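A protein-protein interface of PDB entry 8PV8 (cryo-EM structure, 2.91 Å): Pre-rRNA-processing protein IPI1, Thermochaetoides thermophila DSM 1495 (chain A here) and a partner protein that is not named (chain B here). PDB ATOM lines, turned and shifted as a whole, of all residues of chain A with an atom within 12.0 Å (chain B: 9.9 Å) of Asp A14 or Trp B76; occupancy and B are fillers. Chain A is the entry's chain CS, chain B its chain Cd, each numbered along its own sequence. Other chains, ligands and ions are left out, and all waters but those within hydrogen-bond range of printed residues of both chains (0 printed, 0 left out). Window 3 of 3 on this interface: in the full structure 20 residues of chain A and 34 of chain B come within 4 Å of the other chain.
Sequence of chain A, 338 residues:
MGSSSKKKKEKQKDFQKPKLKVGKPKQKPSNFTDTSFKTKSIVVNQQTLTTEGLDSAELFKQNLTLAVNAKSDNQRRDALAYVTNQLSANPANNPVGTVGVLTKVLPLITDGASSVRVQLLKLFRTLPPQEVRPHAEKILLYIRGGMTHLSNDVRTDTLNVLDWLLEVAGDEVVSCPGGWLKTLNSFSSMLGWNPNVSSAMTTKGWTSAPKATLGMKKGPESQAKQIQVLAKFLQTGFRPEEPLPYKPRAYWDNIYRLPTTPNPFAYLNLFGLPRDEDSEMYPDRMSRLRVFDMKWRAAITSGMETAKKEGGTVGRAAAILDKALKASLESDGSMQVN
The backbone carbonyl oxygen of Thr B80 sits close to the backbone carbonyl oxygen of Ser A30 (3.3 Å).
The backbone carbonyl oxygen (O) of Glu B71 is in hydrogen-bond range of the indole nitrogen (NE1) of Trp B76. The backbone NH (N) of Lys B75 is in hydrogen-bond range of the side-chain amide oxygen (OD1) of Asn B73 (3.1 Å). The backbone carbonyl oxygen (O) of Lys B75 lies within hydrogen-bond range of the side-chain hydroxyl (OG1) of Thr B78.
CZ2 of Trp B76 touches OD2 of Asp A14, 3.8 Å away. CD2 of Phe A15 touches OD1 of Asn B73 (3.3 Å). CD of Lys B75 touches CG of Phe A15 (3.9 Å). Phe A15 touches Trp B76. Asn A31 touches Asn B79. Thr B80 touches Asn A31.
Asp A14 touches just one residue of chain B: Trp B76. Of chain B, only Asn B73, Lys B75 and Trp B76 come within 4 Å of Phe A15. Of the printed residues of chain B, Ser A30 touches Thr B80 (3.3 Å). Of the printed residues of chain B, Asn A31 touches Asn B79 and Thr B80. No residue of chain A comes within 4 Å of Ile B70. No residue of chain A comes within 4 Å of Pro B72. Of chain A, only Phe A15 (3.3 Å) comes within 4 Å of Asn B73. Of chain A, only Phe A15 (3.9 Å) comes within 4 Å of Lys B75. Trp B76 touches just these residues of chain A: Asp A14 (3.8 Å) and Phe A15 (3.5 Å). No residue of chain A comes within 4 Å of Phe B77. No residue of chain A comes within 4 Å of Thr B78. Of the printed residues of chain A, Asn B79 touches Asn A31 (3.7 Å). Of the printed residues of chain A, Thr B80 touches Ser A30 and Asn A31. The nearest residue of chain A that does not touch Trp B76 is Lys A13 (7.8 Å).
Of the 12 printed residues of chain B, 5 touch a printed residue of chain A. Printed residues of chain B that touch a printed residue of chain A: Asn B73, Lys B75, Trp B76, Asn B79 and Thr B80. Among the printed residues, no Asp or Glu carboxylate lies within 4 Å of a Lys or Arg side-chain nitrogen of the other chain.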
ATOM      1  N   LYS A   9     -10.132   3.363   0.452  1.00  0.00           N
ATOM      2  CA  LYS A   9     -10.694   3.755   1.739  1.00  0.00           C
ATOM      3  C   LYS A   9     -11.966   2.970   2.043  1.00  0.00           C
ATOM      4  O   LYS A   9     -12.445   2.959   3.176  1.00  0.00           O
ATOM      5  CB  LYS A   9     -10.984   5.257   1.763  1.00  0.00           C
ATOM      6  N   GLU A  10     -12.509   2.312   1.018  1.00  0.00           N
ATOM      7  CA  GLU A  10     -13.726   1.524   1.174  1.00  0.00           C
ATOM      8  C   GLU A  10     -13.467   0.136   1.741  1.00  0.00           C
ATOM      9  O   GLU A  10     -14.434  -0.581   2.025  1.00  0.00           O
ATOM     10  CB  GLU A  10     -14.448   1.408  -0.169  1.00  0.00           C
ATOM     11  N   LYS A  11     -12.207  -0.264   1.900  1.00  0.00           N
ATOM     12  CA  LYS A  11     -11.899  -1.575   2.456  1.00  0.00           C
ATOM     13  C   LYS A  11     -12.256  -1.625   3.937  1.00  0.00           C
ATOM     14  O   LYS A  11     -12.057  -0.657   4.676  1.00  0.00           O
ATOM     15  CB  LYS A  11     -10.419  -1.900   2.258  1.00  0.00           C
ATOM     16  N   GLN A  12     -12.788  -2.771   4.370  1.00  0.00           N
ATOM     17  CA  GLN A  12     -13.224  -2.974   5.750  1.00  0.00           C
ATOM     18  C   GLN A  12     -12.478  -4.178   6.329  1.00  0.00           C
ATOM     19  O   GLN A  12     -12.915  -5.324   6.206  1.00  0.00           O
ATOM     20  CB  GLN A  12     -14.740  -3.162   5.826  1.00  0.00           C
ATOM     21  CG  GLN A  12     -15.534  -1.921   5.461  1.00  0.00           C
ATOM     22  CD  GLN A  12     -15.286  -0.773   6.417  1.00  0.00           C
ATOM     23  OE1 GLN A  12     -14.665   0.228   6.056  1.00  0.00           O
ATOM     24  NE2 GLN A  12     -15.768  -0.911   7.647  1.00  0.00           N
ATOM     25  N   LYS A  13     -11.340  -3.907   6.963  1.00  0.00           N
ATOM     26  CA  LYS A  13     -10.590  -4.962   7.628  1.00  0.00           C
ATOM     27  C   LYS A  13     -11.297  -5.386   8.911  1.00  0.00           C
ATOM     28  O   LYS A  13     -12.123  -4.654   9.463  1.00  0.00           O
ATOM     29  CB  LYS A  13      -9.170  -4.490   7.943  1.00  0.00           C
ATOM     30  CG  LYS A  13      -8.423  -3.919   6.751  1.00  0.00           C
ATOM     31  CD  LYS A  13      -7.050  -3.408   7.159  1.00  0.00           C
ATOM     32  CE  LYS A  13      -6.287  -2.850   5.968  1.00  0.00           C
ATOM     33  NZ  LYS A  13      -6.090  -3.875   4.906  1.00  0.00           N
ATOM     34  N   ASP A  14     -10.976  -6.598   9.373  1.00  0.00           N
ATOM     35  CA  ASP A  14     -11.531  -7.087  10.630  1.00  0.00           C
ATOM     36  C   ASP A  14     -11.046  -6.265  11.817  1.00  0.00           C
ATOM     37  O   ASP A  14     -11.831  -5.960  12.722  1.00  0.00           O
ATOM     38  CB  ASP A  14     -11.174  -8.560  10.825  1.00  0.00           C
ATOM     39  CG  ASP A  14     -11.707  -9.439   9.713  1.00  0.00           C
ATOM     40  OD1 ASP A  14     -12.741  -9.079   9.114  1.00  0.00           O
ATOM     41  OD2 ASP A  14     -11.090 -10.489   9.437  1.00  0.00           O
ATOM     42  N   PHE A  15      -9.767  -5.898  11.829  1.00  0.00           N
ATOM     43  CA  PHE A  15      -9.196  -5.050  12.862  1.00  0.00           C
ATOM     44  C   PHE A  15      -8.551  -3.838  12.212  1.00  0.00           C
ATOM     45  O   PHE A  15      -7.861  -3.961  11.195  1.00  0.00           O
ATOM     46  CB  PHE A  15      -8.159  -5.802  13.703  1.00  0.00           C
ATOM     47  CG  PHE A  15      -8.718  -6.979  14.443  1.00  0.00           C
ATOM     48  CD1 PHE A  15      -9.268  -6.820  15.704  1.00  0.00           C
ATOM     49  CD2 PHE A  15      -8.694  -8.245  13.882  1.00  0.00           C
ATOM     50  CE1 PHE A  15      -9.782  -7.900  16.391  1.00  0.00           C
ATOM     51  CE2 PHE A  15      -9.208  -9.328  14.563  1.00  0.00           C
ATOM     52  CZ  PHE A  15      -9.752  -9.154  15.820  1.00  0.00           C
ATOM     53  N   GLN A  16      -8.772  -2.669  12.804  1.00  0.00           N
ATOM     54  CA  GLN A  16      -8.223  -1.417  12.304  1.00  0.00           C
ATOM     55  C   GLN A  16      -7.034  -1.023  13.169  1.00  0.00           C
ATOM     56  O   GLN A  16      -7.169  -0.883  14.389  1.00  0.00           O
ATOM     57  CB  GLN A  16      -9.281  -0.313  12.305  1.00  0.00           C
ATOM     58  CG  GLN A  16     -10.498  -0.624  11.452  1.00  0.00           C
ATOM     59  CD  GLN A  16     -11.532   0.482  11.490  1.00  0.00           C
ATOM     60  OE1 GLN A  16     -11.405   1.439  12.254  1.00  0.00           O
ATOM     61  NE2 GLN A  16     -12.564   0.355  10.665  1.00  0.00           N
ATOM     62  N   LYS A  17      -5.878  -0.855  12.538  1.00  0.00           N
ATOM     63  CA  LYS A  17      -4.696  -0.424  13.263  1.00  0.00           C
ATOM     64  C   LYS A  17      -4.829   1.049  13.642  1.00  0.00           C
ATOM     65  O   LYS A  17      -5.123   1.885  12.778  1.00  0.00           O
ATOM     66  CB  LYS A  17      -3.438  -0.635  12.420  1.00  0.00           C
ATOM     67  CG  LYS A  17      -3.288  -2.038  11.863  1.00  0.00           C
ATOM     68  CD  LYS A  17      -1.955  -2.202  11.154  1.00  0.00           C
ATOM     69  CE  LYS A  17      -1.702  -3.654  10.792  1.00  0.00           C
ATOM     70  NZ  LYS A  17      -0.325  -3.862  10.266  1.00  0.00           N
ATOM     71  N   PRO A  18      -4.647   1.397  14.914  1.00  0.00           N
ATOM     72  CA  PRO A  18      -4.666   2.812  15.297  1.00  0.00           C
ATOM     73  C   PRO A  18      -3.483   3.560  14.704  1.00  0.00           C
ATOM     74  O   PRO A  18      -2.390   3.014  14.538  1.00  0.00           O
ATOM     75  CB  PRO A  18      -4.589   2.767  16.827  1.00  0.00           C
ATOM     76  CG  PRO A  18      -3.917   1.470  17.125  1.00  0.00           C
ATOM     77  CD  PRO A  18      -4.378   0.514  16.062  1.00  0.00           C
ATOM     78  N   SER A  30      -6.413  -1.287  23.483  1.00  0.00           N
ATOM     79  CA  SER A  30      -7.720  -1.836  23.134  1.00  0.00           C
ATOM     80  C   SER A  30      -8.281  -2.707  24.252  1.00  0.00           C
ATOM     81  O   SER A  30      -9.499  -2.898  24.345  1.00  0.00           O
ATOM     82  CB  SER A  30      -7.620  -2.632  21.834  1.00  0.00           C
ATOM     83  OG  SER A  30      -6.509  -3.510  21.857  1.00  0.00           O
ATOM     84  N   ASN A  31      -7.413  -3.249  25.108  1.00  0.00           N
ATOM     85  CA  ASN A  31      -7.892  -4.083  26.202  1.00  0.00           C
ATOM     86  C   ASN A  31      -8.140  -3.291  27.478  1.00  0.00           C
ATOM     87  O   ASN A  31      -8.509  -3.884  28.497  1.00  0.00           O
ATOM     88  CB  ASN A  31      -6.913  -5.232  26.463  1.00  0.00           C
ATOM     89  CG  ASN A  31      -5.491  -4.758  26.696  1.00  0.00           C
ATOM     90  OD1 ASN A  31      -5.213  -3.560  26.724  1.00  0.00           O
ATOM     91  ND2 ASN A  31      -4.579  -5.706  26.866  1.00  0.00           N
ATOM     92  N   VAL B  69     -15.447 -16.561   4.567  1.00  0.00           N
ATOM     93  CA  VAL B  69     -14.141 -17.007   5.027  1.00  0.00           C
ATOM     94  C   VAL B  69     -13.640 -16.028   6.078  1.00  0.00           C
ATOM     95  O   VAL B  69     -14.076 -14.874   6.142  1.00  0.00           O
ATOM     96  CB  VAL B  69     -13.120 -17.136   3.872  1.00  0.00           C
ATOM     97  CG1 VAL B  69     -13.638 -18.081   2.800  1.00  0.00           C
ATOM     98  CG2 VAL B  69     -12.803 -15.775   3.275  1.00  0.00           C
ATOM     99  N   ILE B  70     -12.733 -16.507   6.922  1.00  0.00           N
ATOM    100  CA  ILE B  70     -12.086 -15.686   7.937  1.00  0.00           C
ATOM    101  C   ILE B  70     -10.589 -15.754   7.684  1.00  0.00           C
ATOM    102  O   ILE B  70      -9.979 -16.824   7.807  1.00  0.00           O
ATOM    103  CB  ILE B  70     -12.426 -16.146   9.360  1.00  0.00           C
ATOM    104  CG1 ILE B  70     -13.931 -16.023   9.607  1.00  0.00           C
ATOM    105  CG2 ILE B  70     -11.635 -15.337  10.376  1.00  0.00           C
ATOM    106  CD1 ILE B  70     -14.332 -16.214  11.046  1.00  0.00           C
ATOM    107  N   GLU B  71     -10.000 -14.621   7.324  1.00  0.00           N
ATOM    108  CA  GLU B  71      -8.569 -14.577   7.078  1.00  0.00           C
ATOM    109  C   GLU B  71      -7.812 -14.706   8.397  1.00  0.00           C
ATOM    110  O   GLU B  71      -8.307 -14.264   9.439  1.00  0.00           O
ATOM    111  CB  GLU B  71      -8.189 -13.276   6.371  1.00  0.00           C
ATOM    112  CG  GLU B  71      -8.803 -13.121   4.987  1.00  0.00           C
ATOM    113  CD  GLU B  71      -8.232 -14.094   3.969  1.00  0.00           C
ATOM    114  OE1 GLU B  71      -7.083 -14.548   4.148  1.00  0.00           O
ATOM    115  OE2 GLU B  71      -8.938 -14.406   2.987  1.00  0.00           O
ATOM    116  N   PRO B  72      -6.636 -15.332   8.393  1.00  0.00           N
ATOM    117  CA  PRO B  72      -5.855 -15.439   9.632  1.00  0.00           C
ATOM    118  C   PRO B  72      -5.384 -14.077  10.116  1.00  0.00           C
ATOM    119  O   PRO B  72      -4.968 -13.225   9.329  1.00  0.00           O
ATOM    120  CB  PRO B  72      -4.679 -16.337   9.233  1.00  0.00           C
ATOM    121  CG  PRO B  72      -4.603 -16.249   7.752  1.00  0.00           C
ATOM    122  CD  PRO B  72      -6.003 -16.053   7.276  1.00  0.00           C
ATOM    123  N   ASN B  73      -5.452 -13.877  11.429  1.00  0.00           N
ATOM    124  CA  ASN B  73      -5.054 -12.619  12.036  1.00  0.00           C
ATOM    125  C   ASN B  73      -4.517 -12.900  13.429  1.00  0.00           C
ATOM    126  O   ASN B  73      -5.005 -13.788  14.133  1.00  0.00           O
ATOM    127  CB  ASN B  73      -6.219 -11.625  12.095  1.00  0.00           C
ATOM    128  CG  ASN B  73      -5.767 -10.212  12.383  1.00  0.00           C
ATOM    129  OD1 ASN B  73      -5.830  -9.748  13.520  1.00  0.00           O
ATOM    130  ND2 ASN B  73      -5.311  -9.514  11.351  1.00  0.00           N
ATOM    131  N   ARG B  74      -3.499 -12.131  13.818  1.00  0.00           N
ATOM    132  CA  ARG B  74      -2.832 -12.368  15.092  1.00  0.00           C
ATOM    133  C   ARG B  74      -3.680 -11.896  16.269  1.00  0.00           C
ATOM    134  O   ARG B  74      -3.519 -12.395  17.388  1.00  0.00           O
ATOM    135  CB  ARG B  74      -1.464 -11.682  15.074  1.00  0.00           C
ATOM    136  CG  ARG B  74      -0.571 -11.940  16.276  1.00  0.00           C
ATOM    137  CD  ARG B  74       0.816 -11.370  16.038  1.00  0.00           C
ATOM    138  NE  ARG B  74       1.514 -12.074  14.969  1.00  0.00           N
ATOM    139  CZ  ARG B  74       1.808 -11.548  13.789  1.00  0.00           C
ATOM    140  NH1 ARG B  74       1.443 -10.318  13.470  1.00  0.00           N
ATOM    141  NH2 ARG B  74       2.476 -12.279  12.900  1.00  0.00           N
ATOM    142  N   LYS B  75      -4.611 -10.974  16.033  1.00  0.00           N
ATOM    143  CA  LYS B  75      -5.399 -10.398  17.115  1.00  0.00           C
ATOM    144  C   LYS B  75      -6.588 -11.258  17.526  1.00  0.00           C
ATOM    145  O   LYS B  75      -7.309 -10.875  18.453  1.00  0.00           O
ATOM    146  CB  LYS B  75      -5.885  -9.002  16.725  1.00  0.00           C
ATOM    147  CG  LYS B  75      -4.774  -8.070  16.277  1.00  0.00           C
ATOM    148  CD  LYS B  75      -5.241  -6.627  16.229  1.00  0.00           C
ATOM    149  CE  LYS B  75      -5.780  -6.175  17.575  1.00  0.00           C
ATOM    150  NZ  LYS B  75      -6.307  -4.784  17.518  1.00  0.00           N
ATOM    151  N   TRP B  76      -6.820 -12.396  16.870  1.00  0.00           N
ATOM    152  CA  TRP B  76      -7.844 -13.321  17.342  1.00  0.00           C
ATOM    153  C   TRP B  76      -7.439 -14.045  18.617  1.00  0.00           C
ATOM    154  O   TRP B  76      -8.315 -14.557  19.322  1.00  0.00           O
ATOM    155  CB  TRP B  76      -8.174 -14.371  16.274  1.00  0.00           C
ATOM    156  CG  TRP B  76      -8.709 -13.850  14.969  1.00  0.00           C
ATOM    157  CD1 TRP B  76      -8.176 -14.060  13.733  1.00  0.00           C
ATOM    158  CD2 TRP B  76      -9.896 -13.070  14.764  1.00  0.00           C
ATOM    159  NE1 TRP B  76      -8.943 -13.450  12.774  1.00  0.00           N
ATOM    160  CE2 TRP B  76     -10.004 -12.834  13.380  1.00  0.00           C
ATOM    161  CE3 TRP B  76     -10.872 -12.542  15.615  1.00  0.00           C
ATOM    162  CZ2 TRP B  76     -11.046 -12.094  12.828  1.00  0.00           C
ATOM    163  CZ3 TRP B  76     -11.904 -11.806  15.063  1.00  0.00           C
ATOM    164  CH2 TRP B  76     -11.984 -11.590  13.684  1.00  0.00           C
ATOM    165  N   PHE B  77      -6.144 -14.100  18.931  1.00  0.00           N
ATOM    166  CA  PHE B  77      -5.631 -14.892  20.043  1.00  0.00           C
ATOM    167  C   PHE B  77      -5.079 -14.012  21.158  1.00  0.00           C
ATOM    168  O   PHE B  77      -4.141 -14.398  21.856  1.00  0.00           O
ATOM    169  CB  PHE B  77      -4.559 -15.869  19.560  1.00  0.00           C
ATOM    170  CG  PHE B  77      -4.969 -16.679  18.365  1.00  0.00           C
ATOM    171  CD1 PHE B  77      -5.658 -17.868  18.524  1.00  0.00           C
ATOM    172  CD2 PHE B  77      -4.651 -16.262  17.082  1.00  0.00           C
ATOM    173  CE1 PHE B  77      -6.037 -18.618  17.430  1.00  0.00           C
ATOM    174  CE2 PHE B  77      -5.028 -17.006  15.985  1.00  0.00           C
ATOM    175  CZ  PHE B  77      -5.720 -18.187  16.159  1.00  0.00           C
ATOM    176  N   THR B  78      -5.653 -12.827  21.337  1.00  0.00           N
ATOM    177  CA  THR B  78      -5.225 -11.896  22.369  1.00  0.00           C
ATOM    178  C   THR B  78      -6.390 -11.584  23.297  1.00  0.00           C
ATOM    179  O   THR B  78      -7.557 -11.727  22.923  1.00  0.00           O
ATOM    180  CB  THR B  78      -4.693 -10.592  21.765  1.00  0.00           C
ATOM    181  OG1 THR B  78      -5.720  -9.975  20.979  1.00  0.00           O
ATOM    182  CG2 THR B  78      -3.483 -10.861  20.887  1.00  0.00           C
ATOM    183  N   ASN B  79      -6.059 -11.166  24.516  1.00  0.00           N
ATOM    184  CA  ASN B  79      -7.078 -10.692  25.441  1.00  0.00           C
ATOM    185  C   ASN B  79      -7.664  -9.382  24.937  1.00  0.00           C
ATOM    186  O   ASN B  79      -6.936  -8.449  24.587  1.00  0.00           O
ATOM    187  CB  ASN B  79      -6.489 -10.497  26.837  1.00  0.00           C
ATOM    188  CG  ASN B  79      -5.942 -11.780  27.424  1.00  0.00           C
ATOM    189  OD1 ASN B  79      -6.466 -12.863  27.174  1.00  0.00           O
ATOM    190  ND2 ASN B  79      -4.883 -11.663  28.215  1.00  0.00           N
ATOM    191  N   THR B  80      -8.993  -9.311  24.900  1.00  0.00           N
ATOM    192  CA  THR B  80      -9.667  -8.131  24.380  1.00  0.00           C
ATOM    193  C   THR B  80     -10.092  -7.155  25.465  1.00  0.00           C
ATOM    194  O   THR B  80     -10.286  -5.973  25.164  1.00  0.00           O
ATOM    195  CB  THR B  80     -10.903  -8.533  23.569  1.00  0.00           C
ATOM    196  OG1 THR B  80     -11.926  -9.003  24.453  1.00  0.00           O
ATOM    197  CG2 THR B  80     -10.551  -9.638  22.597  1.00  0.00           C
